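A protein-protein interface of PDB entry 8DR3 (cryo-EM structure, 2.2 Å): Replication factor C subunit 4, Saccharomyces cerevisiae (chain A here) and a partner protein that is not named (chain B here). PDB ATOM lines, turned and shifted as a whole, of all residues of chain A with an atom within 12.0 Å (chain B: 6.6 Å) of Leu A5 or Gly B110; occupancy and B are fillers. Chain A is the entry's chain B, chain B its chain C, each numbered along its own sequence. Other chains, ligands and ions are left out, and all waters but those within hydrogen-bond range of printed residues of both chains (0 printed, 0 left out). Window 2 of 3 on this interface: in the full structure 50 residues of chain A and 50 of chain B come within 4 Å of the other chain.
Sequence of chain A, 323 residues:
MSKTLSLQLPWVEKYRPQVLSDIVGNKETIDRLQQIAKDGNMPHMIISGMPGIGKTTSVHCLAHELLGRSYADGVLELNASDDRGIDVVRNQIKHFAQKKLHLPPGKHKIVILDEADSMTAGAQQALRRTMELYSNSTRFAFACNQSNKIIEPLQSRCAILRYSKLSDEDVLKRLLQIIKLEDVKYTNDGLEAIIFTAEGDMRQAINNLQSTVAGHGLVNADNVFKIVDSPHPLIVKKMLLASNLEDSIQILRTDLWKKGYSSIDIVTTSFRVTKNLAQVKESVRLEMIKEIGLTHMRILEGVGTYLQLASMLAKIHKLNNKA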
ATOM      1  N   THR A   4      21.364 -10.939  -2.584  1.00  0.00           N
ATOM      2  CA  THR A   4      22.806 -11.005  -2.788  1.00  0.00           C
ATOM      3  C   THR A   4      23.490  -9.825  -2.105  1.00  0.00           C
ATOM      4  O   THR A   4      23.106  -8.673  -2.306  1.00  0.00           O
ATOM      5  CB  THR A   4      23.166 -11.014  -4.286  1.00  0.00           C
ATOM      6  OG1 THR A   4      22.770 -12.262  -4.869  1.00  0.00           O
ATOM      7  CG2 THR A   4      24.661 -10.817  -4.485  1.00  0.00           C
ATOM      8  N   LEU A   5      24.504 -10.124  -1.296  1.00  0.00           N
ATOM      9  CA  LEU A   5      25.236  -9.114  -0.545  1.00  0.00           C
ATOM     10  C   LEU A   5      26.540  -8.706  -1.220  1.00  0.00           C
ATOM     11  O   LEU A   5      27.302  -7.922  -0.646  1.00  0.00           O
ATOM     12  CB  LEU A   5      25.523  -9.625   0.869  1.00  0.00           C
ATOM     13  CG  LEU A   5      24.301  -9.907   1.749  1.00  0.00           C
ATOM     14  CD1 LEU A   5      24.737 -10.408   3.116  1.00  0.00           C
ATOM     15  CD2 LEU A   5      23.425  -8.671   1.885  1.00  0.00           C
ATOM     16  N   SER A   6      26.813  -9.213  -2.417  1.00  0.00           N
ATOM     17  CA  SER A   6      28.027  -8.890  -3.150  1.00  0.00           C
ATOM     18  C   SER A   6      27.755  -7.787  -4.167  1.00  0.00           C
ATOM     19  O   SER A   6      26.650  -7.668  -4.703  1.00  0.00           O
ATOM     20  CB  SER A   6      28.579 -10.126  -3.864  1.00  0.00           C
ATOM     21  OG  SER A   6      29.393 -10.894  -2.996  1.00  0.00           O
ATOM     22  N   LEU A   7      28.778  -6.978  -4.424  1.00  0.00           N
ATOM     23  CA  LEU A   7      28.702  -5.880  -5.375  1.00  0.00           C
ATOM     24  C   LEU A   7      29.758  -6.061  -6.456  1.00  0.00           C
ATOM     25  O   LEU A   7      30.866  -6.532  -6.182  1.00  0.00           O
ATOM     26  CB  LEU A   7      28.906  -4.526  -4.682  1.00  0.00           C
ATOM     27  CG  LEU A   7      27.725  -3.954  -3.895  1.00  0.00           C
ATOM     28  CD1 LEU A   7      28.138  -2.666  -3.199  1.00  0.00           C
ATOM     29  CD2 LEU A   7      26.524  -3.716  -4.798  1.00  0.00           C
ATOM     30  N   GLN A   8      29.408  -5.684  -7.682  1.00  0.00           N
ATOM     31  CA  GLN A   8      30.345  -5.664  -8.796  1.00  0.00           C
ATOM     32  C   GLN A   8      30.887  -4.249  -8.945  1.00  0.00           C
ATOM     33  O   GLN A   8      30.114  -3.286  -8.998  1.00  0.00           O
ATOM     34  CB  GLN A   8      29.666  -6.126 -10.090  1.00  0.00           C
ATOM     35  CG  GLN A   8      30.438  -5.807 -11.367  1.00  0.00           C
ATOM     36  CD  GLN A   8      29.693  -6.227 -12.619  1.00  0.00           C
ATOM     37  OE1 GLN A   8      28.837  -5.498 -13.120  1.00  0.00           O
ATOM     38  NE2 GLN A   8      30.015  -7.409 -13.131  1.00  0.00           N
ATOM     39  N   LEU A   9      32.207  -4.127  -9.004  1.00  0.00           N
ATOM     40  CA  LEU A   9      32.827  -2.812  -9.046  1.00  0.00           C
ATOM     41  C   LEU A   9      32.360  -2.058 -10.290  1.00  0.00           C
ATOM     42  O   LEU A   9      32.409  -2.613 -11.396  1.00  0.00           O
ATOM     43  CB  LEU A   9      34.350  -2.941  -9.050  1.00  0.00           C
ATOM     44  CG  LEU A   9      35.130  -1.644  -8.821  1.00  0.00           C
ATOM     45  CD1 LEU A   9      34.949  -1.147  -7.395  1.00  0.00           C
ATOM     46  CD2 LEU A   9      36.604  -1.841  -9.139  1.00  0.00           C
ATOM     47  N   VAL B  41      19.701  -7.064  -8.605  1.00  0.00           N
ATOM     48  CA  VAL B  41      19.965  -7.584  -7.267  1.00  0.00           C
ATOM     49  C   VAL B  41      20.320  -9.065  -7.315  1.00  0.00           C
ATOM     50  O   VAL B  41      21.125  -9.543  -6.507  1.00  0.00           O
ATOM     51  CB  VAL B  41      18.758  -7.324  -6.345  1.00  0.00           C
ATOM     52  CG1 VAL B  41      18.793  -8.250  -5.135  1.00  0.00           C
ATOM     53  CG2 VAL B  41      18.733  -5.869  -5.905  1.00  0.00           C
ATOM     54  N   GLY B  44      24.021  -9.455  -8.155  1.00  0.00           N
ATOM     55  CA  GLY B  44      24.932  -8.555  -7.466  1.00  0.00           C
ATOM     56  C   GLY B  44      25.532  -7.490  -8.356  1.00  0.00           C
ATOM     57  O   GLY B  44      26.742  -7.244  -8.297  1.00  0.00           O
ATOM     58  N   ILE B  70      16.916  -7.474  -0.139  1.00  0.00           N
ATOM     59  CA  ILE B  70      18.369  -7.582  -0.043  1.00  0.00           C
ATOM     60  C   ILE B  70      18.781  -8.058   1.344  1.00  0.00           C
ATOM     61  O   ILE B  70      19.628  -8.949   1.485  1.00  0.00           O
ATOM     62  CB  ILE B  70      19.029  -6.236  -0.395  1.00  0.00           C
ATOM     63  CG1 ILE B  70      18.947  -5.979  -1.900  1.00  0.00           C
ATOM     64  CG2 ILE B  70      20.482  -6.217   0.067  1.00  0.00           C
ATOM     65  CD1 ILE B  70      19.136  -4.525  -2.283  1.00  0.00           C
ATOM     66  N   TYR B  71      18.189  -7.477   2.391  1.00  0.00           N
ATOM     67  CA  TYR B  71      18.635  -7.712   3.757  1.00  0.00           C
ATOM     68  C   TYR B  71      17.678  -8.556   4.588  1.00  0.00           C
ATOM     69  O   TYR B  71      18.060  -8.993   5.679  1.00  0.00           O
ATOM     70  CB  TYR B  71      18.859  -6.372   4.474  1.00  0.00           C
ATOM     71  CG  TYR B  71      19.903  -5.491   3.825  1.00  0.00           C
ATOM     72  CD1 TYR B  71      21.255  -5.777   3.949  1.00  0.00           C
ATOM     73  CD2 TYR B  71      19.535  -4.371   3.091  1.00  0.00           C
ATOM     74  CE1 TYR B  71      22.213  -4.973   3.359  1.00  0.00           C
ATOM     75  CE2 TYR B  71      20.483  -3.562   2.498  1.00  0.00           C
ATOM     76  CZ  TYR B  71      21.821  -3.867   2.634  1.00  0.00           C
ATOM     77  OH  TYR B  71      22.768  -3.064   2.045  1.00  0.00           O
ATOM     78  N   MET B  78      20.167  -1.988   8.775  1.00  0.00           N
ATOM     79  CA  MET B  78      21.266  -2.154   7.831  1.00  0.00           C
ATOM     80  C   MET B  78      21.188  -1.172   6.666  1.00  0.00           C
ATOM     81  O   MET B  78      21.938  -1.310   5.694  1.00  0.00           O
ATOM     82  CB  MET B  78      21.298  -3.590   7.307  1.00  0.00           C
ATOM     83  CG  MET B  78      20.731  -4.612   8.285  1.00  0.00           C
ATOM     84  SD  MET B  78      20.835  -6.322   7.717  1.00  0.00           S
ATOM     85  CE  MET B  78      22.535  -6.424   7.166  1.00  0.00           C
ATOM     86  N   ARG B 104      31.856  -0.737   8.131  1.00  0.00           N
ATOM     87  CA  ARG B 104      31.241  -2.022   7.836  1.00  0.00           C
ATOM     88  C   ARG B 104      29.891  -2.148   8.537  1.00  0.00           C
ATOM     89  O   ARG B 104      29.560  -1.392   9.453  1.00  0.00           O
ATOM     90  CB  ARG B 104      32.157  -3.169   8.267  1.00  0.00           C
ATOM     91  CG  ARG B 104      33.330  -3.413   7.333  1.00  0.00           C
ATOM     92  CD  ARG B 104      34.307  -4.427   7.911  1.00  0.00           C
ATOM     93  NE  ARG B 104      35.693  -4.059   7.648  1.00  0.00           N
ATOM     94  CZ  ARG B 104      36.740  -4.562   8.288  1.00  0.00           C
ATOM     95  NH1 ARG B 104      36.600  -5.472   9.238  1.00  0.00           N
ATOM     96  NH2 ARG B 104      37.961  -4.141   7.966  1.00  0.00           N
ATOM     97  N   GLN B 105      29.105  -3.125   8.087  1.00  0.00           N
ATOM     98  CA  GLN B 105      27.821  -3.401   8.714  1.00  0.00           C
ATOM     99  C   GLN B 105      28.025  -4.021  10.091  1.00  0.00           C
ATOM    100  O   GLN B 105      28.950  -4.810  10.303  1.00  0.00           O
ATOM    101  CB  GLN B 105      26.991  -4.337   7.836  1.00  0.00           C
ATOM    102  CG  GLN B 105      26.517  -3.718   6.531  1.00  0.00           C
ATOM    103  CD  GLN B 105      25.105  -3.169   6.618  1.00  0.00           C
ATOM    104  OE1 GLN B 105      24.641  -2.784   7.688  1.00  0.00           O
ATOM    105  NE2 GLN B 105      24.415  -3.132   5.484  1.00  0.00           N
ATOM    106  N   SER B 108      25.785  -7.992   9.452  1.00  0.00           N
ATOM    107  CA  SER B 108      26.272  -8.869   8.400  1.00  0.00           C
ATOM    108  C   SER B 108      27.557  -8.305   7.798  1.00  0.00           C
ATOM    109  O   SER B 108      28.114  -7.312   8.278  1.00  0.00           O
ATOM    110  CB  SER B 108      25.195  -9.058   7.333  1.00  0.00           C
ATOM    111  OG  SER B 108      25.021  -7.875   6.575  1.00  0.00           O
ATOM    112  N   LYS B 109      28.035  -8.957   6.737  1.00  0.00           N
ATOM    113  CA  LYS B 109      29.221  -8.527   6.008  1.00  0.00           C
ATOM    114  C   LYS B 109      28.883  -8.011   4.613  1.00  0.00           C
ATOM    115  O   LYS B 109      29.775  -7.888   3.767  1.00  0.00           O
ATOM    116  CB  LYS B 109      30.227  -9.674   5.915  1.00  0.00           C
ATOM    117  CG  LYS B 109      30.462 -10.403   7.232  1.00  0.00           C
ATOM    118  CD  LYS B 109      29.571 -11.632   7.368  1.00  0.00           C
ATOM    119  CE  LYS B 109      30.154 -12.646   8.342  1.00  0.00           C
ATOM    120  NZ  LYS B 109      29.838 -12.307   9.758  1.00  0.00           N
ATOM    121  N   GLY B 110      27.613  -7.702   4.355  1.00  0.00           N
ATOM    122  CA  GLY B 110      27.190  -7.243   3.050  1.00  0.00           C
ATOM    123  C   GLY B 110      27.427  -5.760   2.844  1.00  0.00           C
ATOM    124  O   GLY B 110      27.898  -5.037   3.721  1.00  0.00           O
ATOM    125  N   PHE B 111      27.082  -5.302   1.642  1.00  0.00           N
ATOM    126  CA  PHE B 111      27.240  -3.898   1.304  1.00  0.00           C
ATOM    127  C   PHE B 111      26.160  -3.064   1.995  1.00  0.00           C
ATOM    128  O   PHE B 111      25.207  -3.585   2.579  1.00  0.00           O
ATOM    129  CB  PHE B 111      27.196  -3.704  -0.212  1.00  0.00           C
ATOM    130  CG  PHE B 111      25.831  -3.890  -0.816  1.00  0.00           C
ATOM    131  CD1 PHE B 111      24.958  -2.822  -0.932  1.00  0.00           C
ATOM    132  CD2 PHE B 111      25.428  -5.131  -1.276  1.00  0.00           C
ATOM    133  CE1 PHE B 111      23.706  -2.991  -1.489  1.00  0.00           C
ATOM    134  CE2 PHE B 111      24.176  -5.306  -1.835  1.00  0.00           C
ATOM    135  CZ  PHE B 111      23.315  -4.234  -1.942  1.00  0.00           C
ATOM    136  N   LYS B 112      26.324  -1.747   1.921  1.00  0.00           N
ATOM    137  CA  LYS B 112      25.490  -0.804   2.651  1.00  0.00           C
ATOM    138  C   LYS B 112      24.646   0.018   1.685  1.00  0.00           C
ATOM    139  O   LYS B 112      25.092   0.348   0.582  1.00  0.00           O
ATOM    140  CB  LYS B 112      26.356   0.114   3.512  1.00  0.00           C
ATOM    141  CG  LYS B 112      27.421  -0.650   4.279  1.00  0.00           C
ATOM    142  CD  LYS B 112      27.868   0.073   5.527  1.00  0.00           C
ATOM    143  CE  LYS B 112      26.845   0.006   6.643  1.00  0.00           C
ATOM    144  NZ  LYS B 112      27.136   1.017   7.695  1.00  0.00           N
ATOM    145  N   ASN B 140      31.938  -0.390  -1.619  1.00  0.00           N
ATOM    146  CA  ASN B 140      31.160  -1.076  -0.597  1.00  0.00           C
ATOM    147  C   ASN B 140      29.801  -0.447  -0.319  1.00  0.00           C
ATOM    148  O   ASN B 140      29.034  -1.014   0.468  1.00  0.00           O
ATOM    149  CB  ASN B 140      31.952  -1.132   0.720  1.00  0.00           C
ATOM    150  CG  ASN B 140      33.175  -2.026   0.629  1.00  0.00           C
ATOM    151  OD1 ASN B 140      34.308  -1.560   0.746  1.00  0.00           O
ATOM    152  ND2 ASN B 140      32.949  -3.317   0.418  1.00  0.00           N
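Hydrophobic or aromatic side chains of chain B within 4 Å of the printed part of chain A: Phe B111. Of the 6 printed residues of chain A, 5 touch a printed residue of chain B. Printed residues of chain A that touch a printed residue of chain B: Thr A4, Leu A5, Ser A6, Leu A7 and Gln A8. Hydrophobic or aromatic side chains of chain A that line the printed part of chain B: Leu A5 and Leu A7. Along chain A the printed residues that touch a printed residue of chain B span positions 4 to 8. Among the printed residues, 11 pairs touch across the chains.
Among the printed residues, merely in contact across the chains: Leu A7 with Phe B111, Thr A4 with Val B41, Ser A6 with Gly B44, Thr A4 with Phe B111, Leu A5 with Gly B110, Leu A7 with Gly B44, Thr A4 with Gly B44, Leu A5 with Ile B70 and Leu A7 with Asn B140.
O of Leu A5 lies close to N of Phe B111 (3.5 Å). O of Gly B44 lies within hydrogen-bond range of N of Gln A8.
Of chain B, only Ile B70 (3.8 Å), Gly B110 (3.6 Å) and Phe B111 (3.4 Å) come within 4 Å of Leu A5. Gly B110 touches just one residue of chain A: Leu A5 (3.6 Å). Gly B44 touches just these residues of chain A: Thr A4 (3.8 Å), Ser A6 (3.4 Å), Leu A7 (3.7 Å) and Gln A8 (3.1 Å). Of chain A, only Leu A5 (3.8 Å) comes within 4 Å of Ile B70. No residue of chain A comes within 4 Å of Tyr B71. No residue of chain A comes within 4 Å of Gln B105. No residue of chain A comes within 4 Å of Ser B108. No residue of chain A comes within 4 Å of Lys B109. Phe B111 touches just these residues of chain A: Thr A4, Leu A5 and Leu A7. No residue of chain A comes within 4 Å of Lys B112. Of the printed residues of chain B, Leu A7 touches Gly B44 (3.7 Å), Phe B111 (3.3 Å) and Asn B140 (3.998 Å). Of the printed residues of chain A, Val B41 touches Thr A4 (3.4 Å). Printed residues of chain A within 4 Å of Asn B140: Leu A7 (3.998 Å). Leu A9 touches none of the printed residues of chain B. The nearest residue of chain B that does not touch Leu A5 is Tyr B71 (4.2 Å). The nearest printed residue of chain B that does not touch Ser A6 is Phe B111 (4.4 Å).
The backbone carbonyl oxygen (O) of Phe B111 sits at hydrogen-bond distance from the side-chain hydroxyl (OH) of Tyr B71 (2.6 Å). NE2 of Gln B105 is in hydrogen-bond range of O of Phe B111. OG of Ser B108 sits at hydrogen-bond distance from N of Gly B110 (3.4 Å). The backbone carbonyl oxygen of Asn B140 is in hydrogen-bond range of the backbone NH of Lys B112, at 3.2 Å.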
